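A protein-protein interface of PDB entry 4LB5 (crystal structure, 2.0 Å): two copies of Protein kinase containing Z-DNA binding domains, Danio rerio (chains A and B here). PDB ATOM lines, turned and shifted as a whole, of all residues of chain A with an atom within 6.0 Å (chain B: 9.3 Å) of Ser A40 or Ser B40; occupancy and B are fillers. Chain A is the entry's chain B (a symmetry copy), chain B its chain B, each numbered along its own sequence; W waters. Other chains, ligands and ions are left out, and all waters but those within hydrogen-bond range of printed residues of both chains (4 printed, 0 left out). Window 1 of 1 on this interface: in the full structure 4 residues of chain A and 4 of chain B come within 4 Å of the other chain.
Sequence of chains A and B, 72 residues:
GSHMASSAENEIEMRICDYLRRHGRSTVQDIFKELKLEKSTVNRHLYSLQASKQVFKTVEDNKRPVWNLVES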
ATOM      1  N   VAL A  28     -22.406  26.749 -25.962  1.00  0.00           N
ATOM      2  CA  VAL A  28     -21.666  25.593 -26.466  1.00  0.00           C
ATOM      3  C   VAL A  28     -22.618  24.409 -26.684  1.00  0.00           C
ATOM      4  O   VAL A  28     -22.443  23.617 -27.612  1.00  0.00           O
ATOM      5  CB  VAL A  28     -20.495  25.211 -25.502  1.00  0.00           C
ATOM      6  CG1 VAL A  28     -21.022  24.654 -24.185  1.00  0.00           C
ATOM      7  CG2 VAL A  28     -19.537  24.238 -26.174  1.00  0.00           C
ATOM      8  N   GLU A  38     -17.701  16.844 -29.640  1.00  0.00           N
ATOM      9  CA  GLU A  38     -17.636  16.917 -28.186  1.00  0.00           C
ATOM     10  C   GLU A  38     -17.708  18.381 -27.762  1.00  0.00           C
ATOM     11  O   GLU A  38     -17.202  19.267 -28.462  1.00  0.00           O
ATOM     12  CB  GLU A  38     -16.355  16.279 -27.633  1.00  0.00           C
ATOM     13  CG  GLU A  38     -16.191  14.779 -27.910  1.00  0.00           C
ATOM     14  CD  GLU A  38     -17.082  13.904 -27.051  1.00  0.00           C
ATOM     15  OE1 GLU A  38     -17.881  14.446 -26.260  1.00  0.00           O
ATOM     16  OE2 GLU A  38     -16.983  12.663 -27.155  1.00  0.00           O
ATOM     17  N   LYS A  39     -18.354  18.623 -26.624  1.00  0.00           N
ATOM     18  CA  LYS A  39     -18.413  19.951 -26.023  1.00  0.00           C
ATOM     19  C   LYS A  39     -17.023  20.554 -25.861  1.00  0.00           C
ATOM     20  O   LYS A  39     -16.811  21.741 -26.108  1.00  0.00           O
ATOM     21  CB  LYS A  39     -19.085  19.879 -24.647  1.00  0.00           C
ATOM     22  CG  LYS A  39     -19.060  21.210 -23.865  1.00  0.00           C
ATOM     23  CD  LYS A  39     -19.907  21.159 -22.588  1.00  0.00           C
ATOM     24  CE  LYS A  39     -19.269  20.266 -21.517  1.00  0.00           C
ATOM     25  NZ  LYS A  39     -18.065  20.888 -20.884  1.00  0.00           N
ATOM     26  N   SER A  40     -16.076  19.735 -25.418  1.00  0.00           N
ATOM     27  CA  SER A  40     -14.709  20.212 -25.197  1.00  0.00           C
ATOM     28  C   SER A  40     -14.030  20.655 -26.495  1.00  0.00           C
ATOM     29  O   SER A  40     -13.298  21.660 -26.519  1.00  0.00           O
ATOM     30  CB  SER A  40     -13.874  19.125 -24.517  1.00  0.00           C
ATOM     31  OG  SER A  40     -13.800  17.977 -25.349  1.00  0.00           O
ATOM     32  N   THR A  41     -14.240  19.896 -27.565  1.00  0.00           N
ATOM     33  CA  THR A  41     -13.674  20.256 -28.869  1.00  0.00           C
ATOM     34  C   THR A  41     -14.215  21.623 -29.280  1.00  0.00           C
ATOM     35  O   THR A  41     -13.464  22.490 -29.732  1.00  0.00           O
ATOM     36  CB  THR A  41     -14.039  19.234 -29.954  1.00  0.00           C
ATOM     37  OG1 THR A  41     -13.758  17.912 -29.473  1.00  0.00           O
ATOM     38  CG2 THR A  41     -13.242  19.486 -31.232  1.00  0.00           C
ATOM     39  N   VAL A  42     -15.517  21.820 -29.098  1.00  0.00           N
ATOM     40  CA  VAL A  42     -16.133  23.078 -29.492  1.00  0.00           C
ATOM     41  C   VAL A  42     -15.645  24.240 -28.634  1.00  0.00           C
ATOM     42  O   VAL A  42     -15.338  25.303 -29.174  1.00  0.00           O
ATOM     43  CB  VAL A  42     -17.673  23.001 -29.502  1.00  0.00           C
ATOM     44  CG1 VAL A  42     -18.266  24.381 -29.761  1.00  0.00           C
ATOM     45  CG2 VAL A  42     -18.141  22.014 -30.578  1.00  0.00           C
ATOM     46  N   ASN A  43     -15.583  24.043 -27.308  1.00  0.00           N
ATOM     47  CA  ASN A  43     -15.085  25.075 -26.404  1.00  0.00           C
ATOM     48  C   ASN A  43     -13.638  25.470 -26.681  1.00  0.00           C
ATOM     49  O   ASN A  43     -13.297  26.657 -26.630  1.00  0.00           O
ATOM     50  CB  ASN A  43     -15.223  24.660 -24.922  1.00  0.00           C
ATOM     51  CG  ASN A  43     -16.476  25.218 -24.276  1.00  0.00           C
ATOM     52  OD1 ASN A  43     -16.987  26.261 -24.692  1.00  0.00           O
ATOM     53  ND2 ASN A  43     -16.975  24.529 -23.247  1.00  0.00           N
ATOM     54  N   ARG A  44     -12.786  24.476 -26.936  1.00  0.00           N
ATOM     55  CA  ARG A  44     -11.400  24.743 -27.321  1.00  0.00           C
ATOM     56  C   ARG A  44     -11.350  25.758 -28.456  1.00  0.00           C
ATOM     57  O   ARG A  44     -10.618  26.753 -28.382  1.00  0.00           O
ATOM     58  CB  ARG A  44     -10.685  23.459 -27.770  1.00  0.00           C
ATOM     59  CG  ARG A  44      -9.279  23.698 -28.374  1.00  0.00           C
ATOM     60  CD  ARG A  44      -8.582  22.347 -28.717  1.00  0.00           C
ATOM     61  NE  ARG A  44      -8.767  21.429 -27.592  1.00  0.00           N
ATOM     62  CZ  ARG A  44      -9.342  20.231 -27.677  1.00  0.00           C
ATOM     63  NH1 ARG A  44      -9.744  19.766 -28.861  1.00  0.00           N
ATOM     64  NH2 ARG A  44      -9.492  19.492 -26.578  1.00  0.00           N
ATOM     65  N   HIS A  45     -12.117  25.500 -29.514  1.00  0.00           N
ATOM     66  CA  HIS A  45     -12.064  26.370 -30.684  1.00  0.00           C
ATOM     67  C   HIS A  45     -12.792  27.688 -30.462  1.00  0.00           C
ATOM     68  O   HIS A  45     -12.361  28.717 -30.971  1.00  0.00           O
ATOM     69  CB  HIS A  45     -12.525  25.643 -31.949  1.00  0.00           C
ATOM     70  CG  HIS A  45     -11.564  24.593 -32.398  1.00  0.00           C
ATOM     71  ND1 HIS A  45     -10.448  24.882 -33.150  1.00  0.00           N
ATOM     72  CD2 HIS A  45     -11.512  23.263 -32.145  1.00  0.00           C
ATOM     73  CE1 HIS A  45      -9.764  23.772 -33.366  1.00  0.00           C
ATOM     74  NE2 HIS A  45     -10.389  22.775 -32.766  1.00  0.00           N
ATOM     75  N   ILE B  12     -14.079   2.647 -29.146  1.00  0.00           N
ATOM     76  CA  ILE B  12     -13.431   3.488 -28.149  1.00  0.00           C
ATOM     77  C   ILE B  12     -13.204   2.722 -26.851  1.00  0.00           C
ATOM     78  O   ILE B  12     -12.132   2.787 -26.249  1.00  0.00           O
ATOM     79  CB  ILE B  12     -14.267   4.744 -27.806  1.00  0.00           C
ATOM     80  CG1 ILE B  12     -14.552   5.581 -29.051  1.00  0.00           C
ATOM     81  CG2 ILE B  12     -13.541   5.579 -26.768  1.00  0.00           C
ATOM     82  CD1 ILE B  12     -13.353   6.312 -29.587  1.00  0.00           C
ATOM     83  N   ILE B  16      -9.715   1.801 -24.942  1.00  0.00           N
ATOM     84  CA  ILE B  16      -9.452   2.231 -23.573  1.00  0.00           C
ATOM     85  C   ILE B  16      -9.028   1.044 -22.715  1.00  0.00           C
ATOM     86  O   ILE B  16      -8.032   1.111 -21.991  1.00  0.00           O
ATOM     87  CB  ILE B  16     -10.667   2.923 -22.960  1.00  0.00           C
ATOM     88  CG1 ILE B  16     -10.915   4.246 -23.685  1.00  0.00           C
ATOM     89  CG2 ILE B  16     -10.450   3.149 -21.470  1.00  0.00           C
ATOM     90  CD1 ILE B  16     -12.193   4.952 -23.265  1.00  0.00           C
ATOM     91  N   VAL B  28      -6.875   9.718 -16.699  1.00  0.00           N
ATOM     92  CA  VAL B  28      -7.471  10.025 -17.998  1.00  0.00           C
ATOM     93  C   VAL B  28      -6.428  10.672 -18.919  1.00  0.00           C
ATOM     94  O   VAL B  28      -6.432  10.455 -20.133  1.00  0.00           O
ATOM     95  CB  VAL B  28      -8.732  10.936 -17.838  1.00  0.00           C
ATOM     96  CG1 VAL B  28      -8.348  12.336 -17.370  1.00  0.00           C
ATOM     97  CG2 VAL B  28      -9.533  10.984 -19.131  1.00  0.00           C
ATOM     98  N   GLN B  29      -5.508  11.426 -18.315  1.00  0.00           N
ATOM     99  CA  GLN B  29      -4.415  12.090 -19.020  1.00  0.00           C
ATOM    100  C   GLN B  29      -3.578  11.138 -19.877  1.00  0.00           C
ATOM    101  O   GLN B  29      -3.390  11.363 -21.075  1.00  0.00           O
ATOM    102  CB  GLN B  29      -3.514  12.772 -17.994  1.00  0.00           C
ATOM    103  CG  GLN B  29      -4.293  13.675 -17.057  1.00  0.00           C
ATOM    104  CD  GLN B  29      -4.765  14.916 -17.768  1.00  0.00           C
ATOM    105  OE1 GLN B  29      -4.039  15.474 -18.591  1.00  0.00           O
ATOM    106  NE2 GLN B  29      -5.987  15.349 -17.475  1.00  0.00           N
ATOM    107  N   PHE B  32      -5.957   9.560 -22.777  1.00  0.00           N
ATOM    108  CA  PHE B  32      -6.416  10.366 -23.905  1.00  0.00           C
ATOM    109  C   PHE B  32      -5.271  10.892 -24.759  1.00  0.00           C
ATOM    110  O   PHE B  32      -5.414  11.037 -25.973  1.00  0.00           O
ATOM    111  CB  PHE B  32      -7.438  11.443 -23.486  1.00  0.00           C
ATOM    112  CG  PHE B  32      -6.840  12.786 -23.079  1.00  0.00           C
ATOM    113  CD1 PHE B  32      -6.405  13.695 -24.034  1.00  0.00           C
ATOM    114  CD2 PHE B  32      -6.796  13.161 -21.741  1.00  0.00           C
ATOM    115  CE1 PHE B  32      -5.877  14.931 -23.659  1.00  0.00           C
ATOM    116  CE2 PHE B  32      -6.284  14.395 -21.355  1.00  0.00           C
ATOM    117  CZ  PHE B  32      -5.819  15.282 -22.315  1.00  0.00           C
ATOM    118  N   LEU B  37      -7.662  10.920 -28.335  1.00  0.00           N
ATOM    119  CA  LEU B  37      -9.097  11.146 -28.193  1.00  0.00           C
ATOM    120  C   LEU B  37      -9.268  12.318 -27.237  1.00  0.00           C
ATOM    121  O   LEU B  37      -8.330  12.665 -26.525  1.00  0.00           O
ATOM    122  CB  LEU B  37      -9.770   9.904 -27.607  1.00  0.00           C
ATOM    123  CG  LEU B  37      -9.715   8.641 -28.465  1.00  0.00           C
ATOM    124  CD1 LEU B  37     -10.249   7.441 -27.700  1.00  0.00           C
ATOM    125  CD2 LEU B  37     -10.473   8.836 -29.778  1.00  0.00           C
ATOM    126  N   GLU B  38     -10.446  12.935 -27.219  1.00  0.00           N
ATOM    127  CA  GLU B  38     -10.704  14.000 -26.258  1.00  0.00           C
ATOM    128  C   GLU B  38     -10.778  13.394 -24.859  1.00  0.00           C
ATOM    129  O   GLU B  38     -11.241  12.261 -24.685  1.00  0.00           O
ATOM    130  CB  GLU B  38     -12.005  14.753 -26.566  1.00  0.00           C
ATOM    131  CG  GLU B  38     -12.039  15.489 -27.913  1.00  0.00           C
ATOM    132  CD  GLU B  38     -11.215  16.761 -27.927  1.00  0.00           C
ATOM    133  OE1 GLU B  38     -10.561  17.071 -26.912  1.00  0.00           O
ATOM    134  OE2 GLU B  38     -11.224  17.467 -28.959  1.00  0.00           O
ATOM    135  N   LYS B  39     -10.301  14.152 -23.875  1.00  0.00           N
ATOM    136  CA  LYS B  39     -10.402  13.769 -22.471  1.00  0.00           C
ATOM    137  C   LYS B  39     -11.836  13.423 -22.088  1.00  0.00           C
ATOM    138  O   LYS B  39     -12.086  12.462 -21.360  1.00  0.00           O
ATOM    139  CB  LYS B  39      -9.911  14.912 -21.574  1.00  0.00           C
ATOM    140  CG  LYS B  39     -10.119  14.660 -20.066  1.00  0.00           C
ATOM    141  CD  LYS B  39      -9.445  15.724 -19.192  1.00  0.00           C
ATOM    142  CE  LYS B  39     -10.161  17.076 -19.287  1.00  0.00           C
ATOM    143  NZ  LYS B  39     -11.472  17.091 -18.569  1.00  0.00           N
ATOM    144  N   SER B  40     -12.781  14.227 -22.560  1.00  0.00           N
ATOM    145  CA  SER B  40     -14.191  14.008 -22.234  1.00  0.00           C
ATOM    146  C   SER B  40     -14.721  12.688 -22.797  1.00  0.00           C
ATOM    147  O   SER B  40     -15.504  11.984 -22.136  1.00  0.00           O
ATOM    148  CB  SER B  40     -15.039  15.173 -22.748  1.00  0.00           C
ATOM    149  OG  SER B  40     -14.934  15.264 -24.161  1.00  0.00           O
ATOM    150  N   THR B  41     -14.328  12.365 -24.025  1.00  0.00           N
ATOM    151  CA  THR B  41     -14.740  11.100 -24.641  1.00  0.00           C
ATOM    152  C   THR B  41     -14.236   9.946 -23.780  1.00  0.00           C
ATOM    153  O   THR B  41     -14.973   8.999 -23.497  1.00  0.00           O
ATOM    154  CB  THR B  41     -14.176  10.944 -26.058  1.00  0.00           C
ATOM    155  OG1 THR B  41     -14.435  12.139 -26.807  1.00  0.00           O
ATOM    156  CG2 THR B  41     -14.813   9.754 -26.772  1.00  0.00           C
ATOM    157  N   VAL B  42     -12.983  10.039 -23.345  1.00  0.00           N
ATOM    158  CA  VAL B  42     -12.399   8.972 -22.549  1.00  0.00           C
ATOM    159  C   VAL B  42     -13.064   8.858 -21.181  1.00  0.00           C
ATOM    160  O   VAL B  42     -13.364   7.746 -20.745  1.00  0.00           O
ATOM    161  CB  VAL B  42     -10.869   9.107 -22.414  1.00  0.00           C
ATOM    162  CG1 VAL B  42     -10.333   8.063 -21.440  1.00  0.00           C
ATOM    163  CG2 VAL B  42     -10.205   8.941 -23.785  1.00  0.00           C
ATOM    164  N   ASN B  43     -13.286   9.996 -20.507  1.00  0.00           N
ATOM    165  CA  ASN B  43     -13.961  10.000 -19.212  1.00  0.00           C
ATOM    166  C   ASN B  43     -15.380   9.447 -19.272  1.00  0.00           C
ATOM    167  O   ASN B  43     -15.797   8.707 -18.374  1.00  0.00           O
ATOM    168  CB  ASN B  43     -13.991  11.410 -18.583  1.00  0.00           C
ATOM    169  CG  ASN B  43     -12.869  11.627 -17.585  1.00  0.00           C
ATOM    170  OD1 ASN B  43     -12.373  10.672 -16.981  1.00  0.00           O
ATOM    171  ND2 ASN B  43     -12.467  12.886 -17.402  1.00  0.00           N
ATOM    172  N   ARG B  44     -16.129   9.834 -20.306  1.00  0.00           N
ATOM    173  CA  ARG B  44     -17.467   9.283 -20.523  1.00  0.00           C
ATOM    174  C   ARG B  44     -17.432   7.761 -20.464  1.00  0.00           C
ATOM    175  O   ARG B  44     -18.226   7.138 -19.749  1.00  0.00           O
ATOM    176  CB  ARG B  44     -18.038   9.714 -21.883  1.00  0.00           C
ATOM    177  CG  ARG B  44     -19.365   9.013 -22.263  1.00  0.00           C
ATOM    178  CD  ARG B  44     -19.928   9.570 -23.604  1.00  0.00           C
ATOM    179  NE  ARG B  44     -19.834  11.030 -23.578  1.00  0.00           N
ATOM    180  CZ  ARG B  44     -19.181  11.766 -24.475  1.00  0.00           C
ATOM    181  NH1 ARG B  44     -18.601  11.179 -25.524  1.00  0.00           N
ATOM    182  NH2 ARG B  44     -19.131  13.090 -24.332  1.00  0.00           N
ATOM    183  N   HIS B  45     -16.519   7.161 -21.227  1.00  0.00           N
ATOM    184  CA  HIS B  45     -16.472   5.706 -21.301  1.00  0.00           C
ATOM    185  C   HIS B  45     -15.861   5.078 -20.056  1.00  0.00           C
ATOM    186  O   HIS B  45     -16.285   4.004 -19.642  1.00  0.00           O
ATOM    187  CB  HIS B  45     -15.807   5.227 -22.594  1.00  0.00           C
ATOM    188  CG  HIS B  45     -16.635   5.495 -23.806  1.00  0.00           C
ATOM    189  ND1 HIS B  45     -17.660   4.665 -24.202  1.00  0.00           N
ATOM    190  CD2 HIS B  45     -16.639   6.535 -24.674  1.00  0.00           C
ATOM    191  CE1 HIS B  45     -18.240   5.166 -25.278  1.00  0.00           C
ATOM    192  NE2 HIS B  45     -17.639   6.302 -25.584  1.00  0.00           N
ATOM    193  N   LEU B  46     -14.899   5.762 -19.435  1.00  0.00           N
ATOM    194  CA  LEU B  46     -14.361   5.293 -18.158  1.00  0.00           C
ATOM    195  C   LEU B  46     -15.475   5.167 -17.125  1.00  0.00           C
ATOM    196  O   LEU B  46     -15.597   4.146 -16.440  1.00  0.00           O
ATOM    197  CB  LEU B  46     -13.254   6.213 -17.636  1.00  0.00           C
ATOM    198  CG  LEU B  46     -11.876   6.045 -18.292  1.00  0.00           C
ATOM    199  CD1 LEU B  46     -10.867   7.008 -17.695  1.00  0.00           C
ATOM    200  CD2 LEU B  46     -11.379   4.612 -18.160  1.00  0.00           C
ATOM    201  N   TYR B  47     -16.292   6.203 -17.002  1.00  0.00           N
ATOM    202  CA  TYR B  47     -17.330   6.159 -15.978  1.00  0.00           C
ATOM    203  C   TYR B  47     -18.430   5.166 -16.386  1.00  0.00           C
ATOM    204  O   TYR B  47     -19.025   4.509 -15.539  1.00  0.00           O
ATOM    205  CB  TYR B  47     -17.873   7.559 -15.661  1.00  0.00           C
ATOM    206  CG  TYR B  47     -16.979   8.374 -14.733  1.00  0.00           C
ATOM    207  CD1 TYR B  47     -15.936   9.151 -15.232  1.00  0.00           C
ATOM    208  CD2 TYR B  47     -17.171   8.351 -13.352  1.00  0.00           C
ATOM    209  CE1 TYR B  47     -15.107   9.901 -14.366  1.00  0.00           C
ATOM    210  CE2 TYR B  47     -16.355   9.087 -12.490  1.00  0.00           C
ATOM    211  CZ  TYR B  47     -15.327   9.857 -13.006  1.00  0.00           C
ATOM    212  OH  TYR B  47     -14.525  10.602 -12.161  1.00  0.00           O
ATOM    213  N   SER B  48     -18.668   5.032 -17.688  1.00  0.00           N
ATOM    214  CA  SER B  48     -19.599   4.017 -18.179  1.00  0.00           C
ATOM    215  C   SER B  48     -19.091   2.612 -17.872  1.00  0.00           C
ATOM    216  O   SER B  48     -19.840   1.749 -17.406  1.00  0.00           O
ATOM    217  CB  SER B  48     -19.810   4.153 -19.688  1.00  0.00           C
ATOM    218  OG  SER B  48     -20.692   3.142 -20.142  1.00  0.00           O
HETATM  219  O   HOH W   1     -16.792  17.279 -24.154  1.00  0.00           O
HETATM  220  O   HOH W   2     -19.285  16.379 -25.126  1.00  0.00           O
HETATM  221  O   HOH W   3      -9.437  16.791 -24.533  1.00  0.00           O
HETATM  222  O   HOH W   4     -12.085  16.810 -23.557  1.00  0.00           O
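Water W2 lies within hydrogen-bond range of the side-chain carboxylate (OE1) of Glu A38 (2.6 Å), the backbone NH (N) of Lys A39 (2.9 Å) and the guanidinium group (NH2) of Arg B44 (3.4 Å).
Water W3 lies within hydrogen-bond range of OE1 of Glu B38, N of Lys B39 and NH2 of Arg A44.
Water W4 lies within hydrogen-bond range of the side-chain hydroxyl (OG) of Ser A40 (2.7 Å), the backbone NH (N) of Ser B40 (2.9 Å) and the backbone NH (N) of Lys B39 (3.2 Å).
Water W1 lies within hydrogen-bond range of OG of Ser B40 (2.7 Å), N of Ser A40 (2.9 Å) and N of Lys A39 (3.2 Å).
Of the 17 printed residues of chain B, 4 touch a printed residue of chain A.
The side-chain carboxylate (OE1) of Glu B38 lies within salt-bridge range of the guanidinium group (NH2) of Arg A44 (2.7 Å).
OE2 of Glu A38 is in hydrogen-bond range of OG1 of Thr B41, at 2.6 Å.
The side-chain hydroxyl (OG1) of Thr A41 sits at hydrogen-bond distance from the side-chain carboxylate (OE2) of Glu B38.
The side-chain hydroxyl (OG) of Ser A40 is in hydrogen-bond range of the side-chain hydroxyl (OG) of Ser B40 (3.2 Å).
The side-chain carboxylate (OE1) of Glu A38 lies within salt-bridge range of the guanidinium group (NH2) of Arg B44 (2.7 Å).
Glu A38 touches Ser B40, and with the chains exchanged Ser A40 touches Glu B38.
Glu A38 touches Thr B41, and with the chains exchanged Thr A41 touches Glu B38.
Glu A38 touches Arg B44, and with the chains exchanged Arg A44 touches Glu B38.
Ser A40 touches its own counterpart, Ser B40.
Positions printed for both chains: 28, 38, 39, 40, 41, 42, 43, 44 and 45.
Glu A38 touches Ser B40 (OE1 to OG, 3.7 Å).
OE1 of Glu B38 touches OG of Ser A40, at 3.7 Å.
Printed residues of chain B within 4 Å of Glu A38: Ser B40, Thr B41 and Arg B44.
Printed residues of chain B within 4 Å of Ser A40: Glu B38 and Ser B40.
Thr A41 touches one residue of chain B.
Printed residues of chain B within 4 Å of Arg A44: Glu B38 (2.7 Å).
Of the printed residues of chain A, Glu B38 touches Ser A40 (3.7 Å), Thr A41 (2.6 Å) and Arg A44 (2.7 Å).
Of chain A, only Glu A38 and Ser A40 come within 4 Å of Ser B40.
Of the printed residues of chain A, Thr B41 touches Glu A38 (2.6 Å).
Of the printed residues of chain A, Arg B44 touches Glu A38.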
